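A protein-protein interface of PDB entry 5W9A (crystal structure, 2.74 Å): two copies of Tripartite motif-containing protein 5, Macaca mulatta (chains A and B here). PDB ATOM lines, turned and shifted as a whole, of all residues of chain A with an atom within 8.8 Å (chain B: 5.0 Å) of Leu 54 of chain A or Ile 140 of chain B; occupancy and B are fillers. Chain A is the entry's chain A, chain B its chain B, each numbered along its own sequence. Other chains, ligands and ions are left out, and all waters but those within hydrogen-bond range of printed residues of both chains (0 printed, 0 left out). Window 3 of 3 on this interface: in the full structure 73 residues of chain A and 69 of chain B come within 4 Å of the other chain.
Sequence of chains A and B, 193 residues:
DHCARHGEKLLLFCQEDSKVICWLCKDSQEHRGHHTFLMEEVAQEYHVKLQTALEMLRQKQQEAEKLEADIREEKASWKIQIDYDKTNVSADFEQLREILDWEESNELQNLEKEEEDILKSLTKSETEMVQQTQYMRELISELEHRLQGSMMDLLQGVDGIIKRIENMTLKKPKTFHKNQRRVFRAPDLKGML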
ATOM      1  N   TYR A  46     -21.542 -30.179 -11.075  1.00  0.00           N
ATOM      2  CA  TYR A  46     -22.136 -28.968 -10.523  1.00  0.00           C
ATOM      3  C   TYR A  46     -21.244 -27.754 -10.747  1.00  0.00           C
ATOM      4  O   TYR A  46     -21.752 -26.637 -10.890  1.00  0.00           O
ATOM      5  CB  TYR A  46     -22.453 -29.162  -9.042  1.00  0.00           C
ATOM      6  CG  TYR A  46     -23.766 -29.883  -8.821  1.00  0.00           C
ATOM      7  CD1 TYR A  46     -24.968 -29.186  -8.834  1.00  0.00           C
ATOM      8  CD2 TYR A  46     -23.806 -31.256  -8.621  1.00  0.00           C
ATOM      9  CE1 TYR A  46     -26.173 -29.834  -8.642  1.00  0.00           C
ATOM     10  CE2 TYR A  46     -25.010 -31.914  -8.428  1.00  0.00           C
ATOM     11  CZ  TYR A  46     -26.188 -31.197  -8.440  1.00  0.00           C
ATOM     12  OH  TYR A  46     -27.388 -31.843  -8.248  1.00  0.00           O
ATOM     13  N   HIS A  47     -19.926 -27.952 -10.827  1.00  0.00           N
ATOM     14  CA  HIS A  47     -19.020 -26.838 -11.079  1.00  0.00           C
ATOM     15  C   HIS A  47     -19.257 -26.243 -12.462  1.00  0.00           C
ATOM     16  O   HIS A  47     -19.402 -25.024 -12.609  1.00  0.00           O
ATOM     17  CB  HIS A  47     -17.573 -27.308 -10.928  1.00  0.00           C
ATOM     18  CG  HIS A  47     -16.570 -26.197 -10.922  1.00  0.00           C
ATOM     19  ND1 HIS A  47     -16.238 -25.503  -9.779  1.00  0.00           N
ATOM     20  CD2 HIS A  47     -15.823 -25.664 -11.917  1.00  0.00           C
ATOM     21  CE1 HIS A  47     -15.331 -24.587 -10.070  1.00  0.00           C
ATOM     22  NE2 HIS A  47     -15.061 -24.665 -11.362  1.00  0.00           N
ATOM     23  N   VAL A  48     -19.315 -27.093 -13.492  1.00  0.00           N
ATOM     24  CA  VAL A  48     -19.541 -26.566 -14.837  1.00  0.00           C
ATOM     25  C   VAL A  48     -20.962 -26.020 -14.977  1.00  0.00           C
ATOM     26  O   VAL A  48     -21.187 -25.018 -15.678  1.00  0.00           O
ATOM     27  CB  VAL A  48     -19.224 -27.631 -15.907  1.00  0.00           C
ATOM     28  CG1 VAL A  48     -17.751 -28.015 -15.851  1.00  0.00           C
ATOM     29  CG2 VAL A  48     -20.103 -28.858 -15.744  1.00  0.00           C
ATOM     30  N   LYS A  49     -21.936 -26.642 -14.304  1.00  0.00           N
ATOM     31  CA  LYS A  49     -23.302 -26.124 -14.331  1.00  0.00           C
ATOM     32  C   LYS A  49     -23.362 -24.715 -13.747  1.00  0.00           C
ATOM     33  O   LYS A  49     -23.956 -23.803 -14.340  1.00  0.00           O
ATOM     34  CB  LYS A  49     -24.224 -27.074 -13.565  1.00  0.00           C
ATOM     35  CG  LYS A  49     -25.708 -26.831 -13.772  1.00  0.00           C
ATOM     36  CD  LYS A  49     -26.529 -27.905 -13.072  1.00  0.00           C
ATOM     37  CE  LYS A  49     -28.019 -27.711 -13.303  1.00  0.00           C
ATOM     38  NZ  LYS A  49     -28.822 -28.747 -12.594  1.00  0.00           N
ATOM     39  N   LEU A  50     -22.725 -24.512 -12.591  1.00  0.00           N
ATOM     40  CA  LEU A  50     -22.713 -23.191 -11.976  1.00  0.00           C
ATOM     41  C   LEU A  50     -21.875 -22.204 -12.778  1.00  0.00           C
ATOM     42  O   LEU A  50     -22.142 -21.001 -12.740  1.00  0.00           O
ATOM     43  CB  LEU A  50     -22.208 -23.287 -10.538  1.00  0.00           C
ATOM     44  CG  LEU A  50     -23.120 -23.990  -9.531  1.00  0.00           C
ATOM     45  CD1 LEU A  50     -22.661 -23.710  -8.108  1.00  0.00           C
ATOM     46  CD2 LEU A  50     -24.570 -23.570  -9.724  1.00  0.00           C
ATOM     47  N   GLN A  51     -20.869 -22.684 -13.512  1.00  0.00           N
ATOM     48  CA  GLN A  51     -20.123 -21.803 -14.407  1.00  0.00           C
ATOM     49  C   GLN A  51     -21.028 -21.249 -15.503  1.00  0.00           C
ATOM     50  O   GLN A  51     -21.024 -20.041 -15.788  1.00  0.00           O
ATOM     51  CB  GLN A  51     -18.937 -22.557 -15.011  1.00  0.00           C
ATOM     52  CG  GLN A  51     -17.972 -21.684 -15.795  1.00  0.00           C
ATOM     53  CD  GLN A  51     -17.064 -20.870 -14.893  1.00  0.00           C
ATOM     54  OE1 GLN A  51     -17.136 -19.642 -14.865  1.00  0.00           O
ATOM     55  NE2 GLN A  51     -16.200 -21.554 -14.151  1.00  0.00           N
ATOM     56  N   THR A  52     -21.811 -22.126 -16.137  1.00  0.00           N
ATOM     57  CA  THR A  52     -22.752 -21.660 -17.154  1.00  0.00           C
ATOM     58  C   THR A  52     -23.797 -20.726 -16.548  1.00  0.00           C
ATOM     59  O   THR A  52     -24.198 -19.730 -17.172  1.00  0.00           O
ATOM     60  CB  THR A  52     -23.426 -22.852 -17.833  1.00  0.00           C
ATOM     61  OG1 THR A  52     -24.130 -23.627 -16.855  1.00  0.00           O
ATOM     62  CG2 THR A  52     -22.389 -23.731 -18.521  1.00  0.00           C
ATOM     63  N   ALA A  53     -24.238 -21.023 -15.321  1.00  0.00           N
ATOM     64  CA  ALA A  53     -25.175 -20.134 -14.638  1.00  0.00           C
ATOM     65  C   ALA A  53     -24.558 -18.761 -14.394  1.00  0.00           C
ATOM     66  O   ALA A  53     -25.229 -17.733 -14.543  1.00  0.00           O
ATOM     67  CB  ALA A  53     -25.630 -20.763 -13.322  1.00  0.00           C
ATOM     68  N   LEU A  54     -23.279 -18.726 -14.009  1.00  0.00           N
ATOM     69  CA  LEU A  54     -22.581 -17.459 -13.814  1.00  0.00           C
ATOM     70  C   LEU A  54     -22.501 -16.668 -15.113  1.00  0.00           C
ATOM     71  O   LEU A  54     -22.655 -15.440 -15.113  1.00  0.00           O
ATOM     72  CB  LEU A  54     -21.182 -17.716 -13.256  1.00  0.00           C
ATOM     73  CG  LEU A  54     -20.273 -16.500 -13.075  1.00  0.00           C
ATOM     74  CD1 LEU A  54     -20.759 -15.632 -11.926  1.00  0.00           C
ATOM     75  CD2 LEU A  54     -18.832 -16.934 -12.852  1.00  0.00           C
ATOM     76  N   GLU A  55     -22.239 -17.354 -16.229  1.00  0.00           N
ATOM     77  CA  GLU A  55     -22.235 -16.682 -17.528  1.00  0.00           C
ATOM     78  C   GLU A  55     -23.587 -16.031 -17.809  1.00  0.00           C
ATOM     79  O   GLU A  55     -23.667 -14.846 -18.185  1.00  0.00           O
ATOM     80  CB  GLU A  55     -21.879 -17.684 -18.628  1.00  0.00           C
ATOM     81  CG  GLU A  55     -21.697 -17.071 -20.007  1.00  0.00           C
ATOM     82  CD  GLU A  55     -20.479 -16.175 -20.094  1.00  0.00           C
ATOM     83  OE1 GLU A  55     -19.510 -16.411 -19.343  1.00  0.00           O
ATOM     84  OE2 GLU A  55     -20.491 -15.234 -20.915  1.00  0.00           O
ATOM     85  N   MET A  56     -24.665 -16.801 -17.632  1.00  0.00           N
ATOM     86  CA  MET A  56     -26.003 -16.260 -17.855  1.00  0.00           C
ATOM     87  C   MET A  56     -26.278 -15.064 -16.949  1.00  0.00           C
ATOM     88  O   MET A  56     -26.859 -14.062 -17.388  1.00  0.00           O
ATOM     89  CB  MET A  56     -27.059 -17.343 -17.634  1.00  0.00           C
ATOM     90  CG  MET A  56     -28.481 -16.803 -17.621  1.00  0.00           C
ATOM     91  SD  MET A  56     -29.699 -17.957 -16.962  1.00  0.00           S
ATOM     92  CE  MET A  56     -31.160 -16.917 -16.933  1.00  0.00           C
ATOM     93  N   LEU A  57     -25.861 -15.146 -15.683  1.00  0.00           N
ATOM     94  CA  LEU A  57     -26.129 -14.055 -14.751  1.00  0.00           C
ATOM     95  C   LEU A  57     -25.335 -12.806 -15.109  1.00  0.00           C
ATOM     96  O   LEU A  57     -25.832 -11.687 -14.946  1.00  0.00           O
ATOM     97  CB  LEU A  57     -25.822 -14.491 -13.319  1.00  0.00           C
ATOM     98  CG  LEU A  57     -26.775 -15.518 -12.707  1.00  0.00           C
ATOM     99  CD1 LEU A  57     -26.361 -15.849 -11.283  1.00  0.00           C
ATOM    100  CD2 LEU A  57     -28.209 -15.012 -12.752  1.00  0.00           C
ATOM    101  N   ARG A  58     -24.103 -12.970 -15.593  1.00  0.00           N
ATOM    102  CA  ARG A  58     -23.334 -11.816 -16.051  1.00  0.00           C
ATOM    103  C   ARG A  58     -24.042 -11.116 -17.205  1.00  0.00           C
ATOM    104  O   ARG A  58     -24.197  -9.883 -17.206  1.00  0.00           O
ATOM    105  CB  ARG A  58     -21.928 -12.253 -16.463  1.00  0.00           C
ATOM    106  N   GLN A  59     -24.488 -11.894 -18.196  1.00  0.00           N
ATOM    107  CA  GLN A  59     -25.204 -11.294 -19.322  1.00  0.00           C
ATOM    108  C   GLN A  59     -26.472 -10.581 -18.857  1.00  0.00           C
ATOM    109  O   GLN A  59     -26.757  -9.450 -19.282  1.00  0.00           O
ATOM    110  CB  GLN A  59     -25.532 -12.362 -20.367  1.00  0.00           C
ATOM    111  CG  GLN A  59     -24.305 -12.977 -21.024  1.00  0.00           C
ATOM    112  CD  GLN A  59     -23.472 -11.955 -21.778  1.00  0.00           C
ATOM    113  OE1 GLN A  59     -24.006 -11.012 -22.363  1.00  0.00           O
ATOM    114  NE2 GLN A  59     -22.157 -12.139 -21.764  1.00  0.00           N
ATOM    115  N   LYS A  60     -27.241 -11.222 -17.971  1.00  0.00           N
ATOM    116  CA  LYS A  60     -28.488 -10.624 -17.506  1.00  0.00           C
ATOM    117  C   LYS A  60     -28.245  -9.367 -16.679  1.00  0.00           C
ATOM    118  O   LYS A  60     -29.036  -8.421 -16.748  1.00  0.00           O
ATOM    119  CB  LYS A  60     -29.290 -11.647 -16.701  1.00  0.00           C
ATOM    120  N   GLN A  61     -27.156  -9.327 -15.907  1.00  0.00           N
ATOM    121  CA  GLN A  61     -26.847  -8.129 -15.131  1.00  0.00           C
ATOM    122  C   GLN A  61     -26.445  -6.973 -16.038  1.00  0.00           C
ATOM    123  O   GLN A  61     -26.822  -5.818 -15.790  1.00  0.00           O
ATOM    124  CB  GLN A  61     -25.742  -8.436 -14.119  1.00  0.00           C
ATOM    125  CG  GLN A  61     -25.438  -7.300 -13.158  1.00  0.00           C
ATOM    126  CD  GLN A  61     -23.951  -7.068 -12.981  1.00  0.00           C
ATOM    127  OE1 GLN A  61     -23.129  -7.679 -13.665  1.00  0.00           O
ATOM    128  NE2 GLN A  61     -23.596  -6.181 -12.058  1.00  0.00           N
ATOM    129  N   GLN A  62     -25.679  -7.261 -17.095  1.00  0.00           N
ATOM    130  CA  GLN A  62     -25.391  -6.230 -18.089  1.00  0.00           C
ATOM    131  C   GLN A  62     -26.681  -5.685 -18.697  1.00  0.00           C
ATOM    132  O   GLN A  62     -26.865  -4.464 -18.823  1.00  0.00           O
ATOM    133  CB  GLN A  62     -24.473  -6.795 -19.173  1.00  0.00           C
ATOM    134  CG  GLN A  62     -24.107  -5.805 -20.264  1.00  0.00           C
ATOM    135  CD  GLN A  62     -23.164  -6.395 -21.294  1.00  0.00           C
ATOM    136  OE1 GLN A  62     -22.656  -7.504 -21.125  1.00  0.00           O
ATOM    137  NE2 GLN A  62     -22.924  -5.655 -22.369  1.00  0.00           N
ATOM    138  N   MET B 136     -28.969  -9.012  -8.799  1.00  0.00           N
ATOM    139  CA  MET B 136     -28.135  -9.736  -9.756  1.00  0.00           C
ATOM    140  C   MET B 136     -26.678  -9.755  -9.307  1.00  0.00           C
ATOM    141  O   MET B 136     -26.009 -10.797  -9.363  1.00  0.00           O
ATOM    142  CB  MET B 136     -28.259  -9.109 -11.147  1.00  0.00           C
ATOM    143  CG  MET B 136     -29.665  -9.132 -11.724  1.00  0.00           C
ATOM    144  SD  MET B 136     -30.266 -10.805 -12.014  1.00  0.00           S
ATOM    145  CE  MET B 136     -29.005 -11.416 -13.125  1.00  0.00           C
ATOM    146  N   ARG B 137     -26.165  -8.602  -8.871  1.00  0.00           N
ATOM    147  CA  ARG B 137     -24.786  -8.547  -8.385  1.00  0.00           C
ATOM    148  C   ARG B 137     -24.589  -9.466  -7.182  1.00  0.00           C
ATOM    149  O   ARG B 137     -23.556 -10.139  -7.062  1.00  0.00           O
ATOM    150  CB  ARG B 137     -24.411  -7.108  -8.030  1.00  0.00           C
ATOM    151  N   GLU B 138     -25.578  -9.509  -6.286  1.00  0.00           N
ATOM    152  CA  GLU B 138     -25.498 -10.377  -5.115  1.00  0.00           C
ATOM    153  C   GLU B 138     -25.426 -11.845  -5.519  1.00  0.00           C
ATOM    154  O   GLU B 138     -24.614 -12.609  -4.981  1.00  0.00           O
ATOM    155  CB  GLU B 138     -26.705 -10.131  -4.212  1.00  0.00           C
ATOM    156  CG  GLU B 138     -26.807 -11.054  -3.010  1.00  0.00           C
ATOM    157  CD  GLU B 138     -28.021 -10.748  -2.153  1.00  0.00           C
ATOM    158  OE1 GLU B 138     -28.705  -9.740  -2.428  1.00  0.00           O
ATOM    159  OE2 GLU B 138     -28.296 -11.520  -1.209  1.00  0.00           O
ATOM    160  N   LEU B 139     -26.268 -12.254  -6.471  1.00  0.00           N
ATOM    161  CA  LEU B 139     -26.243 -13.642  -6.924  1.00  0.00           C
ATOM    162  C   LEU B 139     -24.921 -13.981  -7.603  1.00  0.00           C
ATOM    163  O   LEU B 139     -24.396 -15.092  -7.437  1.00  0.00           O
ATOM    164  CB  LEU B 139     -27.419 -13.911  -7.861  1.00  0.00           C
ATOM    165  CG  LEU B 139     -28.773 -14.102  -7.173  1.00  0.00           C
ATOM    166  CD1 LEU B 139     -29.826 -14.545  -8.174  1.00  0.00           C
ATOM    167  CD2 LEU B 139     -28.656 -15.103  -6.030  1.00  0.00           C
ATOM    168  N   ILE B 140     -24.363 -13.038  -8.368  1.00  0.00           N
ATOM    169  CA  ILE B 140     -23.075 -13.283  -9.013  1.00  0.00           C
ATOM    170  C   ILE B 140     -21.982 -13.478  -7.967  1.00  0.00           C
ATOM    171  O   ILE B 140     -21.147 -14.389  -8.076  1.00  0.00           O
ATOM    172  CB  ILE B 140     -22.735 -12.137  -9.984  1.00  0.00           C
ATOM    173  CG1 ILE B 140     -23.661 -12.180 -11.201  1.00  0.00           C
ATOM    174  CG2 ILE B 140     -21.279 -12.215 -10.419  1.00  0.00           C
ATOM    175  CD1 ILE B 140     -23.371 -11.105 -12.226  1.00  0.00           C
ATOM    176  N   SER B 141     -21.974 -12.632  -6.933  1.00  0.00           N
ATOM    177  CA  SER B 141     -20.985 -12.781  -5.869  1.00  0.00           C
ATOM    178  C   SER B 141     -21.146 -14.115  -5.149  1.00  0.00           C
ATOM    179  O   SER B 141     -20.153 -14.771  -4.806  1.00  0.00           O
ATOM    180  CB  SER B 141     -21.096 -11.619  -4.881  1.00  0.00           C
ATOM    181  OG  SER B 141     -22.289 -11.708  -4.123  1.00  0.00           O
ATOM    182  N   GLU B 142     -22.393 -14.534  -4.913  1.00  0.00           N
ATOM    183  CA  GLU B 142     -22.628 -15.815  -4.250  1.00  0.00           C
ATOM    184  C   GLU B 142     -22.114 -16.979  -5.090  1.00  0.00           C
ATOM    185  O   GLU B 142     -21.489 -17.906  -4.561  1.00  0.00           O
ATOM    186  CB  GLU B 142     -24.116 -15.990  -3.952  1.00  0.00           C
ATOM    187  CG  GLU B 142     -24.455 -17.310  -3.277  1.00  0.00           C
ATOM    188  CD  GLU B 142     -25.897 -17.382  -2.819  1.00  0.00           C
ATOM    189  OE1 GLU B 142     -26.630 -16.390  -3.002  1.00  0.00           O
ATOM    190  OE2 GLU B 142     -26.296 -18.436  -2.276  1.00  0.00           O
ATOM    191  N   LEU B 143     -22.366 -16.951  -6.402  1.00  0.00           N
ATOM    192  CA  LEU B 143     -21.867 -18.025  -7.258  1.00  0.00           C
ATOM    193  C   LEU B 143     -20.343 -18.036  -7.306  1.00  0.00           C
ATOM    194  O   LEU B 143     -19.725 -19.110  -7.324  1.00  0.00           O
ATOM    195  CB  LEU B 143     -22.447 -17.901  -8.666  1.00  0.00           C
ATOM    196  CG  LEU B 143     -23.895 -18.366  -8.829  1.00  0.00           C
ATOM    197  CD1 LEU B 143     -24.224 -18.576 -10.298  1.00  0.00           C
ATOM    198  CD2 LEU B 143     -24.144 -19.638  -8.033  1.00  0.00           C
ATOM    199  N   GLU B 144     -19.717 -16.856  -7.322  1.00  0.00           N
ATOM    200  CA  GLU B 144     -18.259 -16.804  -7.268  1.00  0.00           C
ATOM    201  C   GLU B 144     -17.737 -17.447  -5.988  1.00  0.00           C
ATOM    202  O   GLU B 144     -16.809 -18.270  -6.020  1.00  0.00           O
ATOM    203  CB  GLU B 144     -17.779 -15.356  -7.377  1.00  0.00           C
ATOM    204  N   LEU B 147     -17.911 -21.135  -6.227  1.00  0.00           N
ATOM    205  CA  LEU B 147     -16.950 -21.760  -7.128  1.00  0.00           C
ATOM    206  C   LEU B 147     -15.508 -21.627  -6.662  1.00  0.00           C
ATOM    207  O   LEU B 147     -14.639 -22.315  -7.210  1.00  0.00           O
ATOM    208  CB  LEU B 147     -17.083 -21.179  -8.537  1.00  0.00           C
ATOM    209  CG  LEU B 147     -18.034 -21.932  -9.469  1.00  0.00           C
ATOM    210  CD1 LEU B 147     -19.460 -21.852  -8.961  1.00  0.00           C
ATOM    211  CD2 LEU B 147     -17.939 -21.397 -10.893  1.00  0.00           C
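Leu 147 of chain B touches Leu 50 of chain A. CD1 of Leu 54 of chain A touches CG2 of Ile 140 of chain B (3.8 Å). Leu 54 of chain A touches Leu 143 of chain B. CE of Met 136 of chain B touches O of Leu 57 of chain A, 3.7 Å away. O of Leu 57 of chain A touches CD1 of Ile 140 of chain B (3.7 Å). CD1 of Leu 57 of chain A touches CD1 of Leu 143 of chain B (3.6 Å). Arg 58 of chain A touches Ile 140 of chain B. CB of Lys 60 of chain A touches CE of Met 136 of chain B (3.6 Å). CB of Met 136 of chain B touches CG of Gln 61 of chain A (3.9 Å). Gln 61 of chain A touches Ile 140 of chain B.
Of the printed residues of chain B, Ala 53 of chain A touches Leu 143. Printed residues of chain B within 4 Å of Leu 54 of chain A: Ile 140 (3.8 Å) and Leu 143 (3.8 Å). Of the printed residues of chain B, Leu 57 of chain A touches Met 136 (3.7 Å), Ile 140 (3.7 Å) and Leu 143 (3.6 Å). Printed residues of chain B within 4 Å of Gln 61 of chain A: Met 136 and Ile 140. Printed residues of chain A within 4 Å of Met 136 of chain B: Leu 57 (3.7 Å), Lys 60 (3.6 Å) and Gln 61 (3.9 Å). Of the printed residues of chain A, Ile 140 of chain B touches Leu 54 (3.8 Å), Leu 57 (3.7 Å), Arg 58 (3.9 Å) and Gln 61 (3.7 Å). No residue of chain A comes within 4 Å of Ser 141 of chain B. Glu 142 of chain B touches none of the printed residues of chain A. Printed residues of chain A within 4 Å of Leu 143 of chain B: Ala 53 (3.99 Å), Leu 54 (3.8 Å) and Leu 57 (3.6 Å). The nearest residue of chain B that does not touch Leu 54 of chain A is Glu 144 of chain B (4.9 Å).
Of the 10 printed residues of chain B, 4 touch a printed residue of chain A. Printed residues of chain B that touch a printed residue of chain A: Met 136, Ile 140, Leu 143 and Leu 147. Of the 17 printed residues of chain A, 9 touch a printed residue of chain B. Printed residues of chain A that touch a printed residue of chain B: His 47, Leu 50, Gln 51, Ala 53, Leu 54, Leu 57, Arg 58, Lys 60 and Gln 61. Hydrophobic or aromatic side chains of chain A within 4 Å of the printed part of chain B: His 47, Leu 50, Ala 53, Leu 54 and Leu 57. Along chain A the printed residues that touch a printed residue of chain B span positions 47 to 61. Among the printed residues, 13 pairs touch across the chains. Among the printed residues, no Asp or Glu carboxylate lies within 4 Å of a Lys or Arg side-chain nitrogen of the other chain.
No position is printed for both chains. Of the 13 pairs that touch across the chains among the printed residues, none has its exchanged pair printed and touching as well.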
